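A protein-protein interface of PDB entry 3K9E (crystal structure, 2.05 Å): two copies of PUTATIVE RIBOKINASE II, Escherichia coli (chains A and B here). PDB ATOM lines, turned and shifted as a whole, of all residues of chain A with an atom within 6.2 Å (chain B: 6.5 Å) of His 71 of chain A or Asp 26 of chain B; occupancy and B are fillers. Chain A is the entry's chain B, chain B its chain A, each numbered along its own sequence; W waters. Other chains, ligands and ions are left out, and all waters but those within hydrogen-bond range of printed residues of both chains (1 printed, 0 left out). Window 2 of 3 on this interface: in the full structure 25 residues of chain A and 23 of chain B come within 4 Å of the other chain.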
ATOM      1  N   PRO A  34     -23.313  18.367 -30.747  1.00  0.00           N
ATOM      2  CA  PRO A  34     -23.560  16.987 -30.320  1.00  0.00           C
ATOM      3  C   PRO A  34     -24.325  16.933 -28.995  1.00  0.00           C
ATOM      4  O   PRO A  34     -24.383  17.923 -28.266  1.00  0.00           O
ATOM      5  CB  PRO A  34     -22.148  16.422 -30.179  1.00  0.00           C
ATOM      6  CG  PRO A  34     -21.378  17.609 -29.694  1.00  0.00           C
ATOM      7  CD  PRO A  34     -21.884  18.701 -30.626  1.00  0.00           C
ATOM      8  N   GLY A  64     -13.387  16.150 -28.966  1.00  0.00           N
ATOM      9  CA  GLY A  64     -14.412  16.905 -28.266  1.00  0.00           C
ATOM     10  C   GLY A  64     -15.707  16.155 -28.029  1.00  0.00           C
ATOM     11  O   GLY A  64     -16.401  16.407 -27.042  1.00  0.00           O
ATOM     12  N   PHE A  65     -16.049  15.247 -28.939  1.00  0.00           N
ATOM     13  CA  PHE A  65     -17.267  14.459 -28.801  1.00  0.00           C
ATOM     14  C   PHE A  65     -17.111  13.535 -27.597  1.00  0.00           C
ATOM     15  O   PHE A  65     -18.067  13.281 -26.854  1.00  0.00           O
ATOM     16  CB  PHE A  65     -17.511  13.635 -30.066  1.00  0.00           C
ATOM     17  CG  PHE A  65     -17.937  14.453 -31.255  1.00  0.00           C
ATOM     18  CD1 PHE A  65     -18.333  15.782 -31.106  1.00  0.00           C
ATOM     19  CD2 PHE A  65     -17.977  13.884 -32.521  1.00  0.00           C
ATOM     20  CE1 PHE A  65     -18.763  16.530 -32.205  1.00  0.00           C
ATOM     21  CE2 PHE A  65     -18.405  14.617 -33.625  1.00  0.00           C
ATOM     22  CZ  PHE A  65     -18.798  15.937 -33.472  1.00  0.00           C
ATOM     23  N   GLY A  66     -15.897  13.027 -27.413  1.00  0.00           N
ATOM     24  CA  GLY A  66     -15.637  12.162 -26.285  1.00  0.00           C
ATOM     25  C   GLY A  66     -15.664  12.988 -25.010  1.00  0.00           C
ATOM     26  O   GLY A  66     -16.162  12.533 -23.980  1.00  0.00           O
ATOM     27  N   ASP A  67     -15.139  14.213 -25.082  1.00  0.00           N
ATOM     28  CA  ASP A  67     -15.102  15.094 -23.918  1.00  0.00           C
ATOM     29  C   ASP A  67     -16.487  15.508 -23.422  1.00  0.00           C
ATOM     30  O   ASP A  67     -16.741  15.499 -22.218  1.00  0.00           O
ATOM     31  CB  ASP A  67     -14.285  16.359 -24.210  1.00  0.00           C
ATOM     32  CG  ASP A  67     -12.831  16.063 -24.563  1.00  0.00           C
ATOM     33  OD1 ASP A  67     -12.294  15.011 -24.150  1.00  0.00           O
ATOM     34  OD2 ASP A  67     -12.214  16.907 -25.246  1.00  0.00           O
ATOM     35  N   ILE A  68     -17.384  15.866 -24.337  1.00  0.00           N
ATOM     36  CA  ILE A  68     -18.719  16.297 -23.936  1.00  0.00           C
ATOM     37  C   ILE A  68     -19.448  15.210 -23.137  1.00  0.00           C
ATOM     38  O   ILE A  68     -20.207  15.507 -22.213  1.00  0.00           O
ATOM     39  CB  ILE A  68     -19.559  16.734 -25.169  1.00  0.00           C
ATOM     40  CG1 ILE A  68     -20.885  17.339 -24.703  1.00  0.00           C
ATOM     41  CG2 ILE A  68     -19.790  15.556 -26.102  1.00  0.00           C
ATOM     42  CD1 ILE A  68     -21.689  17.982 -25.818  1.00  0.00           C
ATOM     43  N   ASN A  69     -19.202  13.951 -23.473  1.00  0.00           N
ATOM     44  CA  ASN A  69     -19.831  12.863 -22.741  1.00  0.00           C
ATOM     45  C   ASN A  69     -19.210  12.764 -21.349  1.00  0.00           C
ATOM     46  O   ASN A  69     -19.922  12.765 -20.344  1.00  0.00           O
ATOM     47  CB  ASN A  69     -19.653  11.542 -23.490  1.00  0.00           C
ATOM     48  CG  ASN A  69     -20.671  11.361 -24.598  1.00  0.00           C
ATOM     49  OD1 ASN A  69     -21.856  11.137 -24.336  1.00  0.00           O
ATOM     50  ND2 ASN A  69     -20.221  11.467 -25.840  1.00  0.00           N
ATOM     51  N   ILE A  70     -17.883  12.686 -21.295  1.00  0.00           N
ATOM     52  CA  ILE A  70     -17.184  12.592 -20.018  1.00  0.00           C
ATOM     53  C   ILE A  70     -17.544  13.749 -19.089  1.00  0.00           C
ATOM     54  O   ILE A  70     -17.784  13.541 -17.901  1.00  0.00           O
ATOM     55  CB  ILE A  70     -15.653  12.567 -20.221  1.00  0.00           C
ATOM     56  CG1 ILE A  70     -15.247  11.257 -20.896  1.00  0.00           C
ATOM     57  CG2 ILE A  70     -14.941  12.723 -18.879  1.00  0.00           C
ATOM     58  CD1 ILE A  70     -13.786  11.190 -21.278  1.00  0.00           C
ATOM     59  N   HIS A  71     -17.589  14.962 -19.634  1.00  0.00           N
ATOM     60  CA  HIS A  71     -17.918  16.150 -18.848  1.00  0.00           C
ATOM     61  C   HIS A  71     -19.315  16.060 -18.244  1.00  0.00           C
ATOM     62  O   HIS A  71     -19.503  16.315 -17.055  1.00  0.00           O
ATOM     63  CB  HIS A  71     -17.835  17.409 -19.717  1.00  0.00           C
ATOM     64  CG  HIS A  71     -16.447  17.752 -20.182  1.00  0.00           C
ATOM     65  ND1 HIS A  71     -16.206  18.686 -21.159  1.00  0.00           N
ATOM     66  CD2 HIS A  71     -15.236  17.292 -19.778  1.00  0.00           C
ATOM     67  CE1 HIS A  71     -14.895  18.797 -21.344  1.00  0.00           C
ATOM     68  NE2 HIS A  71     -14.292  17.966 -20.522  1.00  0.00           N
ATOM     69  N   ARG A  72     -20.291  15.710 -19.077  1.00  0.00           N
ATOM     70  CA  ARG A  72     -21.681  15.586 -18.654  1.00  0.00           C
ATOM     71  C   ARG A  72     -21.827  14.543 -17.548  1.00  0.00           C
ATOM     72  O   ARG A  72     -22.427  14.802 -16.501  1.00  0.00           O
ATOM     73  CB  ARG A  72     -22.569  15.200 -19.854  1.00  0.00           C
ATOM     74  CG  ARG A  72     -23.963  14.701 -19.476  1.00  0.00           C
ATOM     75  CD  ARG A  72     -24.793  15.776 -18.795  1.00  0.00           C
ATOM     76  NE  ARG A  72     -25.523  16.590 -19.759  1.00  0.00           N
ATOM     77  CZ  ARG A  72     -26.719  16.275 -20.251  1.00  0.00           C
ATOM     78  NH1 ARG A  72     -27.331  15.161 -19.870  1.00  0.00           N
ATOM     79  NH2 ARG A  72     -27.304  17.076 -21.129  1.00  0.00           N
ATOM     80  N   LEU A  73     -21.283  13.357 -17.786  1.00  0.00           N
ATOM     81  CA  LEU A  73     -21.369  12.294 -16.801  1.00  0.00           C
ATOM     82  C   LEU A  73     -20.685  12.700 -15.488  1.00  0.00           C
ATOM     83  O   LEU A  73     -21.280  12.580 -14.416  1.00  0.00           O
ATOM     84  CB  LEU A  73     -20.752  11.013 -17.367  1.00  0.00           C
ATOM     85  CG  LEU A  73     -21.685   9.970 -18.014  1.00  0.00           C
ATOM     86  CD1 LEU A  73     -23.015  10.562 -18.422  1.00  0.00           C
ATOM     87  CD2 LEU A  73     -20.975   9.357 -19.207  1.00  0.00           C
ATOM     88  N   ALA A  74     -19.456  13.202 -15.579  1.00  0.00           N
ATOM     89  CA  ALA A  74     -18.706  13.618 -14.390  1.00  0.00           C
ATOM     90  C   ALA A  74     -19.446  14.694 -13.619  1.00  0.00           C
ATOM     91  O   ALA A  74     -19.581  14.608 -12.400  1.00  0.00           O
ATOM     92  CB  ALA A  74     -17.321  14.124 -14.784  1.00  0.00           C
ATOM     93  N   ALA A  75     -19.935  15.704 -14.324  1.00  0.00           N
ATOM     94  CA  ALA A  75     -20.662  16.786 -13.670  1.00  0.00           C
ATOM     95  C   ALA A  75     -21.917  16.271 -12.966  1.00  0.00           C
ATOM     96  O   ALA A  75     -22.285  16.758 -11.889  1.00  0.00           O
ATOM     97  CB  ALA A  75     -21.039  17.859 -14.693  1.00  0.00           C
ATOM     98  N   ASP A  76     -22.574  15.282 -13.566  1.00  0.00           N
ATOM     99  CA  ASP A  76     -23.785  14.730 -12.976  1.00  0.00           C
ATOM    100  C   ASP A  76     -23.498  13.823 -11.773  1.00  0.00           C
ATOM    101  O   ASP A  76     -24.421  13.362 -11.094  1.00  0.00           O
ATOM    102  CB  ASP A  76     -24.597  13.993 -14.044  1.00  0.00           C
ATOM    103  CG  ASP A  76     -25.367  14.945 -14.953  1.00  0.00           C
ATOM    104  OD1 ASP A  76     -25.416  16.156 -14.645  1.00  0.00           O
ATOM    105  OD2 ASP A  76     -25.940  14.489 -15.968  1.00  0.00           O
ATOM    106  N   ILE A  80     -16.323   8.531 -13.574  1.00  0.00           N
ATOM    107  CA  ILE A  80     -15.911   8.342 -14.963  1.00  0.00           C
ATOM    108  C   ILE A  80     -14.554   7.698 -15.203  1.00  0.00           C
ATOM    109  O   ILE A  80     -14.111   7.598 -16.343  1.00  0.00           O
ATOM    110  CB  ILE A  80     -15.967   9.683 -15.732  1.00  0.00           C
ATOM    111  CG1 ILE A  80     -15.099  10.742 -15.036  1.00  0.00           C
ATOM    112  CG2 ILE A  80     -17.407  10.175 -15.788  1.00  0.00           C
ATOM    113  CD1 ILE A  80     -13.600  10.526 -15.181  1.00  0.00           C
ATOM    114  N   PRO B  24     -17.319  25.322 -30.388  1.00  0.00           N
ATOM    115  CA  PRO B  24     -16.610  24.119 -29.941  1.00  0.00           C
ATOM    116  C   PRO B  24     -17.228  22.784 -30.363  1.00  0.00           C
ATOM    117  O   PRO B  24     -18.364  22.720 -30.824  1.00  0.00           O
ATOM    118  CB  PRO B  24     -16.600  24.283 -28.427  1.00  0.00           C
ATOM    119  CG  PRO B  24     -17.936  24.875 -28.177  1.00  0.00           C
ATOM    120  CD  PRO B  24     -18.052  25.934 -29.264  1.00  0.00           C
ATOM    121  N   PHE B  25     -16.451  21.718 -30.205  1.00  0.00           N
ATOM    122  CA  PHE B  25     -16.911  20.374 -30.533  1.00  0.00           C
ATOM    123  C   PHE B  25     -17.577  19.730 -29.312  1.00  0.00           C
ATOM    124  O   PHE B  25     -18.332  18.767 -29.450  1.00  0.00           O
ATOM    125  CB  PHE B  25     -15.736  19.482 -30.952  1.00  0.00           C
ATOM    126  CG  PHE B  25     -15.243  19.718 -32.355  1.00  0.00           C
ATOM    127  CD1 PHE B  25     -16.126  19.725 -33.426  1.00  0.00           C
ATOM    128  CD2 PHE B  25     -13.883  19.869 -32.608  1.00  0.00           C
ATOM    129  CE1 PHE B  25     -15.665  19.879 -34.733  1.00  0.00           C
ATOM    130  CE2 PHE B  25     -13.409  20.023 -33.917  1.00  0.00           C
ATOM    131  CZ  PHE B  25     -14.305  20.026 -34.980  1.00  0.00           C
ATOM    132  N   ASP B  26     -17.303  20.259 -28.121  1.00  0.00           N
ATOM    133  CA  ASP B  26     -17.846  19.675 -26.897  1.00  0.00           C
ATOM    134  C   ASP B  26     -19.025  20.393 -26.242  1.00  0.00           C
ATOM    135  O   ASP B  26     -19.214  20.300 -25.031  1.00  0.00           O
ATOM    136  CB  ASP B  26     -16.727  19.505 -25.865  1.00  0.00           C
ATOM    137  CG  ASP B  26     -16.122  20.825 -25.439  1.00  0.00           C
ATOM    138  OD1 ASP B  26     -16.701  21.880 -25.768  1.00  0.00           O
ATOM    139  OD2 ASP B  26     -15.074  20.811 -24.762  1.00  0.00           O
ATOM    140  N   GLN B  27     -19.811  21.108 -27.037  1.00  0.00           N
ATOM    141  CA  GLN B  27     -20.982  21.817 -26.533  1.00  0.00           C
ATOM    142  C   GLN B  27     -22.055  21.661 -27.599  1.00  0.00           C
ATOM    143  O   GLN B  27     -21.756  21.672 -28.795  1.00  0.00           O
ATOM    144  CB  GLN B  27     -20.695  23.315 -26.341  1.00  0.00           C
ATOM    145  CG  GLN B  27     -19.512  23.660 -25.434  1.00  0.00           C
ATOM    146  CD  GLN B  27     -19.912  23.890 -23.988  1.00  0.00           C
ATOM    147  OE1 GLN B  27     -20.481  23.011 -23.336  1.00  0.00           O
ATOM    148  NE2 GLN B  27     -19.614  25.082 -23.477  1.00  0.00           N
ATOM    149  N   PRO B  28     -23.319  21.511 -27.182  1.00  0.00           N
ATOM    150  CA  PRO B  28     -24.433  21.359 -28.125  1.00  0.00           C
ATOM    151  C   PRO B  28     -24.546  22.612 -28.991  1.00  0.00           C
ATOM    152  O   PRO B  28     -24.609  23.721 -28.465  1.00  0.00           O
ATOM    153  CB  PRO B  28     -25.646  21.207 -27.208  1.00  0.00           C
ATOM    154  CG  PRO B  28     -25.061  20.635 -25.933  1.00  0.00           C
ATOM    155  CD  PRO B  28     -23.786  21.422 -25.788  1.00  0.00           C
HETATM  156  O   HOH W   1     -18.776  19.639 -22.241  1.00  0.00           O
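O of Asp 67 of chain A lies close to ND1 of His 71 of chain A (3.4 Å).
The side-chain amide nitrogen of Asn 69 of chain A lies within hydrogen-bond range of the backbone carbonyl oxygen of Phe 65 of chain A (3.0 Å).
Phe 25 of chain B touches Pro 34 of chain A (O to CG, 3.3 Å).
Pro 34 of chain A touches Gln 27 of chain B (CD to O, 3.5 Å).
Pro 28 of chain B touches Pro 34 of chain A.
Gly 64 of chain A touches Phe 25 of chain B (O to O, 3.9 Å).
O of Gly 64 of chain A touches CB of Asp 26 of chain B, 3.3 Å away.
Phe 65 of chain A touches Phe 25 of chain B.
O of Asp 26 of chain B touches CG1 of Ile 68 of chain A, 3.4 Å away.
N of Gln 27 of chain B touches CD1 of Ile 68 of chain A, at 3.8 Å.
OD2 of Asp 26 of chain B touches CE1 of His 71 of chain A, 3.97 Å away.
Of chain A, only Gly 64 (3.3 Å), Ile 68 (3.4 Å) and His 71 (3.97 Å) come within 4 Å of Asp 26 of chain B.
Of the printed residues of chain B, Phe 65 of chain A touches Phe 25.
Of the printed residues of chain B, Gly 64 of chain A touches Phe 25 (3.9 Å) and Asp 26 (3.3 Å).
Of the printed residues of chain B, Ile 68 of chain A touches Asp 26 (3.4 Å) and Gln 27 (3.8 Å).
Printed residues of chain A within 4 Å of Phe 25 of chain B: Pro 34 (3.3 Å), Gly 64 (3.9 Å) and Phe 65 (3.4 Å).
Printed residues of chain A within 4 Å of Pro 28 of chain B: Pro 34 (3.4 Å).
The nearest residue of chain A that does not touch Asp 26 of chain B is Asp 67 of chain A (4.3 Å).
Printed residues of chain A that touch a printed residue of chain B: Pro 34, Gly 64, Phe 65, Ile 68 and His 71.
Of the 5 printed residues of chain B, 4 touch a printed residue of chain A.
Printed residues of chain B that touch a printed residue of chain A: Phe 25, Asp 26, Gln 27 and Pro 28.
Along chain B the printed residues that touch a printed residue of chain A span positions 25 to 28.
No position is printed for both chains.
Of the 9 pairs that touch across the chains among the printed residues, none has its exchanged pair printed and touching as well.
Water W1 bridges the backbone carbonyl oxygen of Asp 26 of chain B (2.9 Å) and a ring nitrogen (ND1) of His 71 of chain A (2.9 Å).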
